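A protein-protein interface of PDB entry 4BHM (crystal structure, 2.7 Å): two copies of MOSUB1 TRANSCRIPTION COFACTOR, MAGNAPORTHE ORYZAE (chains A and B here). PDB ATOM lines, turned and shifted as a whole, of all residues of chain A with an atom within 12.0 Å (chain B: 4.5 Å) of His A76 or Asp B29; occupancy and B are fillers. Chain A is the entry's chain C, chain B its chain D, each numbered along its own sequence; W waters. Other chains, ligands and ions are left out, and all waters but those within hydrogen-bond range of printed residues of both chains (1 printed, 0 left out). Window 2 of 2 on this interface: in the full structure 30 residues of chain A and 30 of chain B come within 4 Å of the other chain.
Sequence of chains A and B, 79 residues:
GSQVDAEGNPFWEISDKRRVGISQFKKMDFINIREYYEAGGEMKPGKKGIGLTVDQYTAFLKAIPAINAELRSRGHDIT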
ATOM      1  N   SER A  15      11.234   2.474 -15.316  1.00  0.00           N
ATOM      2  CA  SER A  15      11.265   1.431 -14.303  1.00  0.00           C
ATOM      3  C   SER A  15      11.925   0.244 -14.947  1.00  0.00           C
ATOM      4  O   SER A  15      12.506   0.380 -16.013  1.00  0.00           O
ATOM      5  CB  SER A  15       9.862   1.020 -13.909  1.00  0.00           C
ATOM      6  OG  SER A  15       9.464   1.677 -12.737  1.00  0.00           O
ATOM      7  N   ARG A  18       8.220  -0.889 -16.426  1.00  0.00           N
ATOM      8  CA  ARG A  18       7.269   0.151 -16.808  1.00  0.00           C
ATOM      9  C   ARG A  18       7.835   1.109 -17.858  1.00  0.00           C
ATOM     10  O   ARG A  18       8.975   1.566 -17.741  1.00  0.00           O
ATOM     11  CB  ARG A  18       6.790   0.924 -15.597  1.00  0.00           C
ATOM     12  CG  ARG A  18       5.651   0.288 -14.852  1.00  0.00           C
ATOM     13  CD  ARG A  18       5.449   0.999 -13.482  1.00  0.00           C
ATOM     14  NE  ARG A  18       4.439   0.316 -12.683  1.00  0.00           N
ATOM     15  CZ  ARG A  18       3.575   0.913 -11.884  1.00  0.00           C
ATOM     16  NH1 ARG A  18       3.592   2.221 -11.751  1.00  0.00           N
ATOM     17  NH2 ARG A  18       2.691   0.197 -11.223  1.00  0.00           N
ATOM     18  N   ILE A  64       1.683  19.518 -14.847  1.00  0.00           N
ATOM     19  CA  ILE A  64       2.996  19.156 -14.311  1.00  0.00           C
ATOM     20  C   ILE A  64       3.659  20.177 -13.364  1.00  0.00           C
ATOM     21  O   ILE A  64       4.218  19.787 -12.337  1.00  0.00           O
ATOM     22  CB  ILE A  64       3.970  18.690 -15.429  1.00  0.00           C
ATOM     23  CG1 ILE A  64       3.569  17.288 -15.925  1.00  0.00           C
ATOM     24  CG2 ILE A  64       5.424  18.713 -14.941  1.00  0.00           C
ATOM     25  CD1 ILE A  64       4.472  16.721 -17.019  1.00  0.00           C
ATOM     26  N   PRO A  65       3.590  21.480 -13.685  1.00  0.00           N
ATOM     27  CA  PRO A  65       4.188  22.433 -12.730  1.00  0.00           C
ATOM     28  C   PRO A  65       3.507  22.407 -11.357  1.00  0.00           C
ATOM     29  O   PRO A  65       4.167  22.546 -10.322  1.00  0.00           O
ATOM     30  CB  PRO A  65       3.966  23.790 -13.398  1.00  0.00           C
ATOM     31  CG  PRO A  65       3.767  23.484 -14.846  1.00  0.00           C
ATOM     32  CD  PRO A  65       3.126  22.145 -14.921  1.00  0.00           C
ATOM     33  N   ALA A  66       2.194  22.226 -11.345  1.00  0.00           N
ATOM     34  CA  ALA A  66       1.471  22.166 -10.083  1.00  0.00           C
ATOM     35  C   ALA A  66       1.799  20.887  -9.314  1.00  0.00           C
ATOM     36  O   ALA A  66       1.978  20.918  -8.103  1.00  0.00           O
ATOM     37  CB  ALA A  66      -0.017  22.282 -10.323  1.00  0.00           C
ATOM     38  N   ILE A  67       1.864  19.764 -10.024  1.00  0.00           N
ATOM     39  CA  ILE A  67       2.242  18.483  -9.428  1.00  0.00           C
ATOM     40  C   ILE A  67       3.654  18.537  -8.833  1.00  0.00           C
ATOM     41  O   ILE A  67       3.891  18.083  -7.704  1.00  0.00           O
ATOM     42  CB  ILE A  67       2.199  17.349 -10.479  1.00  0.00           C
ATOM     43  CG1 ILE A  67       0.757  17.013 -10.836  1.00  0.00           C
ATOM     44  CG2 ILE A  67       2.916  16.098  -9.965  1.00  0.00           C
ATOM     45  CD1 ILE A  67       0.622  16.351 -12.171  1.00  0.00           C
ATOM     46  N   ASN A  68       4.576  19.086  -9.619  1.00  0.00           N
ATOM     47  CA  ASN A  68       5.957  19.221  -9.218  1.00  0.00           C
ATOM     48  C   ASN A  68       6.077  20.003  -7.913  1.00  0.00           C
ATOM     49  O   ASN A  68       6.780  19.594  -6.990  1.00  0.00           O
ATOM     50  CB  ASN A  68       6.751  19.877 -10.343  1.00  0.00           C
ATOM     51  CG  ASN A  68       7.194  18.874 -11.399  1.00  0.00           C
ATOM     52  OD1 ASN A  68       6.793  17.708 -11.372  1.00  0.00           O
ATOM     53  ND2 ASN A  68       8.039  19.317 -12.321  1.00  0.00           N
ATOM     54  N   ALA A  69       5.342  21.107  -7.833  1.00  0.00           N
ATOM     55  CA  ALA A  69       5.364  21.961  -6.661  1.00  0.00           C
ATOM     56  C   ALA A  69       4.849  21.246  -5.414  1.00  0.00           C
ATOM     57  O   ALA A  69       5.431  21.374  -4.326  1.00  0.00           O
ATOM     58  CB  ALA A  69       4.574  23.225  -6.918  1.00  0.00           C
ATOM     59  N   GLU A  70       3.760  20.502  -5.563  1.00  0.00           N
ATOM     60  CA  GLU A  70       3.160  19.843  -4.417  1.00  0.00           C
ATOM     61  C   GLU A  70       4.079  18.738  -3.885  1.00  0.00           C
ATOM     62  O   GLU A  70       4.205  18.545  -2.665  1.00  0.00           O
ATOM     63  CB  GLU A  70       1.765  19.320  -4.763  1.00  0.00           C
ATOM     64  CG  GLU A  70       1.036  18.606  -3.608  1.00  0.00           C
ATOM     65  CD  GLU A  70       1.068  19.367  -2.269  1.00  0.00           C
ATOM     66  OE1 GLU A  70       1.062  20.622  -2.256  1.00  0.00           O
ATOM     67  OE2 GLU A  70       1.086  18.694  -1.216  1.00  0.00           O
ATOM     68  N   LEU A  71       4.751  18.046  -4.805  1.00  0.00           N
ATOM     69  CA  LEU A  71       5.684  17.002  -4.416  1.00  0.00           C
ATOM     70  C   LEU A  71       6.824  17.546  -3.545  1.00  0.00           C
ATOM     71  O   LEU A  71       7.081  17.036  -2.465  1.00  0.00           O
ATOM     72  CB  LEU A  71       6.208  16.253  -5.646  1.00  0.00           C
ATOM     73  CG  LEU A  71       5.564  14.875  -5.923  1.00  0.00           C
ATOM     74  CD1 LEU A  71       4.261  14.690  -5.170  1.00  0.00           C
ATOM     75  CD2 LEU A  71       5.329  14.607  -7.418  1.00  0.00           C
ATOM     76  N   ARG A  72       7.487  18.591  -4.022  1.00  0.00           N
ATOM     77  CA  ARG A  72       8.543  19.249  -3.275  1.00  0.00           C
ATOM     78  C   ARG A  72       8.119  19.607  -1.846  1.00  0.00           C
ATOM     79  O   ARG A  72       8.824  19.323  -0.886  1.00  0.00           O
ATOM     80  CB  ARG A  72       8.982  20.516  -4.012  1.00  0.00           C
ATOM     81  CG  ARG A  72       9.571  20.273  -5.367  1.00  0.00           C
ATOM     82  CD  ARG A  72      10.206  21.538  -5.884  1.00  0.00           C
ATOM     83  NE  ARG A  72      10.704  21.381  -7.249  1.00  0.00           N
ATOM     84  CZ  ARG A  72      10.079  21.839  -8.334  1.00  0.00           C
ATOM     85  NH1 ARG A  72       8.932  22.489  -8.213  1.00  0.00           N
ATOM     86  NH2 ARG A  72      10.609  21.645  -9.535  1.00  0.00           N
ATOM     87  N   SER A  73       6.949  20.217  -1.723  1.00  0.00           N
ATOM     88  CA  SER A  73       6.376  20.554  -0.432  1.00  0.00           C
ATOM     89  C   SER A  73       6.255  19.342   0.487  1.00  0.00           C
ATOM     90  O   SER A  73       6.136  19.491   1.698  1.00  0.00           O
ATOM     91  CB  SER A  73       5.010  21.199  -0.644  1.00  0.00           C
ATOM     92  OG  SER A  73       4.310  21.352   0.572  1.00  0.00           O
ATOM     93  N   ARG A  74       6.279  18.148  -0.093  1.00  0.00           N
ATOM     94  CA  ARG A  74       6.221  16.904   0.663  1.00  0.00           C
ATOM     95  C   ARG A  74       7.602  16.276   0.798  1.00  0.00           C
ATOM     96  O   ARG A  74       7.718  15.151   1.265  1.00  0.00           O
ATOM     97  CB  ARG A  74       5.294  15.896  -0.020  1.00  0.00           C
ATOM     98  CG  ARG A  74       3.857  16.351  -0.134  1.00  0.00           C
ATOM     99  CD  ARG A  74       3.059  15.508  -1.135  1.00  0.00           C
ATOM    100  NE  ARG A  74       1.674  15.969  -1.199  1.00  0.00           N
ATOM    101  CZ  ARG A  74       0.607  15.199  -1.017  1.00  0.00           C
ATOM    102  NH1 ARG A  74       0.754  13.909  -0.769  1.00  0.00           N
ATOM    103  NH2 ARG A  74      -0.608  15.727  -1.088  1.00  0.00           N
ATOM    104  N   GLY A  75       8.637  16.985   0.359  1.00  0.00           N
ATOM    105  CA  GLY A  75      10.004  16.552   0.566  1.00  0.00           C
ATOM    106  C   GLY A  75      10.526  15.601  -0.484  1.00  0.00           C
ATOM    107  O   GLY A  75      11.095  14.552  -0.166  1.00  0.00           O
ATOM    108  N   HIS A  76      10.326  15.958  -1.750  1.00  0.00           N
ATOM    109  CA  HIS A  76      10.889  15.196  -2.855  1.00  0.00           C
ATOM    110  C   HIS A  76      11.734  16.100  -3.739  1.00  0.00           C
ATOM    111  O   HIS A  76      11.447  17.282  -3.888  1.00  0.00           O
ATOM    112  CB  HIS A  76       9.788  14.509  -3.661  1.00  0.00           C
ATOM    113  CG  HIS A  76       8.939  13.582  -2.853  1.00  0.00           C
ATOM    114  ND1 HIS A  76       9.298  12.276  -2.594  1.00  0.00           N
ATOM    115  CD2 HIS A  76       7.742  13.765  -2.247  1.00  0.00           C
ATOM    116  CE1 HIS A  76       8.360  11.698  -1.868  1.00  0.00           C
ATOM    117  NE2 HIS A  76       7.406  12.578  -1.644  1.00  0.00           N
ATOM    118  N   ASP A  77      12.788  15.542  -4.314  1.00  0.00           N
ATOM    119  CA  ASP A  77      13.700  16.322  -5.139  1.00  0.00           C
ATOM    120  C   ASP A  77      13.348  16.194  -6.619  1.00  0.00           C
ATOM    121  O   ASP A  77      13.839  15.309  -7.311  1.00  0.00           O
ATOM    122  CB  ASP A  77      15.152  15.890  -4.891  1.00  0.00           C
ATOM    123  CG  ASP A  77      16.095  17.077  -4.683  1.00  0.00           C
ATOM    124  OD1 ASP A  77      16.210  17.554  -3.530  1.00  0.00           O
ATOM    125  OD2 ASP A  77      16.728  17.527  -5.667  1.00  0.00           O
ATOM    126  N   ILE A  78      12.499  17.096  -7.091  1.00  0.00           N
ATOM    127  CA  ILE A  78      12.065  17.116  -8.481  1.00  0.00           C
ATOM    128  C   ILE A  78      12.893  18.104  -9.293  1.00  0.00           C
ATOM    129  O   ILE A  78      12.770  19.319  -9.126  1.00  0.00           O
ATOM    130  CB  ILE A  78      10.594  17.553  -8.595  1.00  0.00           C
ATOM    131  CG1 ILE A  78       9.781  17.078  -7.388  1.00  0.00           C
ATOM    132  CG2 ILE A  78       9.993  17.052  -9.887  1.00  0.00           C
ATOM    133  CD1 ILE A  78       9.429  15.620  -7.417  1.00  0.00           C
ATOM    134  N   THR A  79      13.721  17.580 -10.189  1.00  0.00           N
ATOM    135  CA  THR A  79      14.538  18.413 -11.067  1.00  0.00           C
ATOM    136  C   THR A  79      13.837  18.629 -12.411  1.00  0.00           C
ATOM    137  O   THR A  79      13.090  19.593 -12.593  1.00  0.00           O
ATOM    138  CB  THR A  79      15.918  17.770 -11.314  1.00  0.00           C
ATOM    139  OG1 THR A  79      15.930  17.128 -12.594  1.00  0.00           O
ATOM    140  CG2 THR A  79      16.230  16.741 -10.235  1.00  0.00           C
ATOM    141  N   SER B  23      -1.832  11.032  -4.520  1.00  0.00           N
ATOM    142  CA  SER B  23      -2.435  10.466  -3.323  1.00  0.00           C
ATOM    143  C   SER B  23      -1.364   9.973  -2.355  1.00  0.00           C
ATOM    144  O   SER B  23      -0.216   9.733  -2.734  1.00  0.00           O
ATOM    145  CB  SER B  23      -3.405   9.329  -3.670  1.00  0.00           C
ATOM    146  OG  SER B  23      -2.728   8.102  -3.930  1.00  0.00           O
ATOM    147  N   GLN B  24      -1.752   9.835  -1.094  1.00  0.00           N
ATOM    148  CA  GLN B  24      -0.884   9.230  -0.105  1.00  0.00           C
ATOM    149  C   GLN B  24      -1.485   7.930   0.362  1.00  0.00           C
ATOM    150  O   GLN B  24      -2.576   7.903   0.944  1.00  0.00           O
ATOM    151  CB  GLN B  24      -0.656  10.148   1.097  1.00  0.00           C
ATOM    152  CG  GLN B  24       0.688  10.825   1.078  1.00  0.00           C
ATOM    153  CD  GLN B  24       1.055  11.413   2.403  1.00  0.00           C
ATOM    154  OE1 GLN B  24       0.522  11.021   3.444  1.00  0.00           O
ATOM    155  NE2 GLN B  24       1.976  12.362   2.383  1.00  0.00           N
ATOM    156  N   LYS B  27       1.717   6.784   4.147  1.00  0.00           N
ATOM    157  CA  LYS B  27       2.826   7.749   4.194  1.00  0.00           C
ATOM    158  C   LYS B  27       3.564   7.894   2.837  1.00  0.00           C
ATOM    159  O   LYS B  27       4.502   8.680   2.700  1.00  0.00           O
ATOM    160  N   MET B  28       3.122   7.164   1.817  1.00  0.00           N
ATOM    161  CA  MET B  28       3.847   7.156   0.545  1.00  0.00           C
ATOM    162  C   MET B  28       3.073   7.869  -0.559  1.00  0.00           C
ATOM    163  O   MET B  28       1.852   7.761  -0.643  1.00  0.00           O
ATOM    164  CB  MET B  28       4.188   5.726   0.127  1.00  0.00           C
ATOM    165  CG  MET B  28       5.279   5.642  -0.930  1.00  0.00           C
ATOM    166  SD  MET B  28       5.500   3.968  -1.571  1.00  0.00           S
ATOM    167  CE  MET B  28       6.656   4.243  -2.916  1.00  0.00           C
ATOM    168  N   ASP B  29       3.787   8.601  -1.406  1.00  0.00           N
ATOM    169  CA  ASP B  29       3.132   9.387  -2.449  1.00  0.00           C
ATOM    170  C   ASP B  29       3.111   8.714  -3.836  1.00  0.00           C
ATOM    171  O   ASP B  29       4.095   8.099  -4.276  1.00  0.00           O
ATOM    172  CB  ASP B  29       3.743  10.785  -2.530  1.00  0.00           C
ATOM    173  CG  ASP B  29       3.743  11.500  -1.185  1.00  0.00           C
ATOM    174  OD1 ASP B  29       2.743  12.175  -0.845  1.00  0.00           O
ATOM    175  OD2 ASP B  29       4.751  11.375  -0.457  1.00  0.00           O
ATOM    176  N   PHE B  30       1.966   8.823  -4.505  1.00  0.00           N
ATOM    177  CA  PHE B  30       1.805   8.266  -5.835  1.00  0.00           C
ATOM    178  C   PHE B  30       1.184   9.291  -6.749  1.00  0.00           C
ATOM    179  O   PHE B  30       0.318  10.071  -6.342  1.00  0.00           O
ATOM    180  CB  PHE B  30       0.937   7.007  -5.803  1.00  0.00           C
ATOM    181  CG  PHE B  30       1.497   5.920  -4.938  1.00  0.00           C
ATOM    182  CD1 PHE B  30       2.453   5.050  -5.431  1.00  0.00           C
ATOM    183  CD2 PHE B  30       1.090   5.787  -3.620  1.00  0.00           C
ATOM    184  CE1 PHE B  30       2.973   4.068  -4.625  1.00  0.00           C
ATOM    185  CE2 PHE B  30       1.604   4.817  -2.827  1.00  0.00           C
ATOM    186  CZ  PHE B  30       2.543   3.955  -3.323  1.00  0.00           C
ATOM    187  N   ILE B  31       1.632   9.285  -7.993  1.00  0.00           N
ATOM    188  CA  ILE B  31       1.047  10.154  -8.988  1.00  0.00           C
ATOM    189  C   ILE B  31       0.149   9.270  -9.824  1.00  0.00           C
ATOM    190  O   ILE B  31       0.625   8.390 -10.523  1.00  0.00           O
ATOM    191  CB  ILE B  31       2.112  10.838  -9.874  1.00  0.00           C
ATOM    192  CG1 ILE B  31       2.990  11.798  -9.052  1.00  0.00           C
ATOM    193  CG2 ILE B  31       1.428  11.642 -10.964  1.00  0.00           C
ATOM    194  CD1 ILE B  31       3.974  11.162  -8.050  1.00  0.00           C
ATOM    195  N   LEU B  52       1.882   5.869 -10.262  1.00  0.00           N
ATOM    196  CA  LEU B  52       3.309   6.037 -10.435  1.00  0.00           C
ATOM    197  C   LEU B  52       3.954   6.397  -9.121  1.00  0.00           C
ATOM    198  O   LEU B  52       3.412   7.180  -8.339  1.00  0.00           O
ATOM    199  CB  LEU B  52       3.595   7.128 -11.469  1.00  0.00           C
ATOM    200  CG  LEU B  52       3.330   6.832 -12.950  1.00  0.00           C
ATOM    201  CD1 LEU B  52       3.797   8.003 -13.820  1.00  0.00           C
ATOM    202  CD2 LEU B  52       3.992   5.517 -13.415  1.00  0.00           C
ATOM    203  N   THR B  53       5.116   5.812  -8.871  1.00  0.00           N
ATOM    204  CA  THR B  53       5.914   6.229  -7.738  1.00  0.00           C
ATOM    205  C   THR B  53       6.600   7.521  -8.136  1.00  0.00           C
ATOM    206  O   THR B  53       6.630   7.875  -9.319  1.00  0.00           O
ATOM    207  CB  THR B  53       6.979   5.199  -7.379  1.00  0.00           C
ATOM    208  OG1 THR B  53       7.943   5.124  -8.434  1.00  0.00           O
ATOM    209  CG2 THR B  53       6.346   3.860  -7.145  1.00  0.00           C
ATOM    210  N   VAL B  54       7.144   8.221  -7.148  1.00  0.00           N
ATOM    211  CA  VAL B  54       7.868   9.458  -7.388  1.00  0.00           C
ATOM    212  C   VAL B  54       9.062   9.250  -8.327  1.00  0.00           C
ATOM    213  O   VAL B  54       9.210   9.981  -9.316  1.00  0.00           O
ATOM    214  CB  VAL B  54       8.305  10.118  -6.052  1.00  0.00           C
ATOM    215  CG1 VAL B  54       9.182  11.323  -6.304  1.00  0.00           C
ATOM    216  CG2 VAL B  54       7.087  10.521  -5.248  1.00  0.00           C
HETATM  217  O   HOH W   1      -2.497  12.990  -1.325  1.00  0.00           O
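NH1 of Arg A74 is in salt-bridge range of OD1 of Asp B29. The side-chain carboxylate (OD2) of Asp B29 sits at hydrogen-bond distance from a ring nitrogen (NE2) of His A76, 3.1 Å away.
Of the printed residues of chain B, Arg A18 touches Leu B52 (3.7 Å). Of the printed residues of chain B, Arg A74 touches Gln B24 and Asp B29. His A76 touches just these residues of chain B: Asp B29 and Val B54. No residue of chain A comes within 4 Å of Ser B23. Gln B24 touches one residue of chain A. No residue of chain A comes within 4 Å of Lys B27. Of the printed residues of chain A, Asp B29 touches Arg A74 and His A76. No residue of chain A comes within 4 Å of Phe B30. Of chain A, only Leu A71 comes within 4 Å of Ile B31. No residue of chain A comes within 4 Å of Thr B53. Of chain A, only His A76 (3.8 Å) comes within 4 Å of Val B54. The nearest residue of chain A that does not touch Asp B29 is Leu A71 (4.7 Å).
Of the 18 printed residues of chain A, 4 touch a printed residue of chain B. Hydrophobic or aromatic side chains of chain A within 4 Å of the printed part of chain B: Leu A71 and His A76. Printed residues of chain B that touch a printed residue of chain A: Gln B24, Asp B29, Ile B31, Leu B52 and Val B54. Hydrophobic or aromatic side chains of chain B that line the printed part of chain A: Ile B31, Leu B52 and Val B54. Among the printed residues, 6 pairs touch across the chains. Among the printed residues, Asp or Glu carboxylates within 4 Å of a Lys or Arg side-chain nitrogen of the other chain: Arg A74 with Asp B29 (2.6 Å).
No position is printed for both chains. Of the 6 pairs that touch across the chains among the printed residues, none has its exchanged pair printed and touching as well.
Water W1 lies within hydrogen-bond range of the backbone NH of Gln B24 and the guanidinium group of Arg A74.
N of His A76 lies close to O of Leu A71 (3.5 Å). The guanidinium group of Arg A74 lies within salt-bridge range of the side-chain carboxylate of Glu A70 (2.8 Å). The backbone NH of Ile B31 is in hydrogen-bond range of the backbone carbonyl oxygen of Leu B52 (2.8 Å). NE2 of Gln B24 lies close to OD1 of Asp B29.
NH1 of Arg A18 touches CD2 of Leu B52, 3.7 Å away. Ile B31 touches Leu A71 (CD1 to CD2, 3.8 Å). Gln B24 touches Arg A74 (CG to NH1, 3.6 Å). Val B54 touches His A76.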
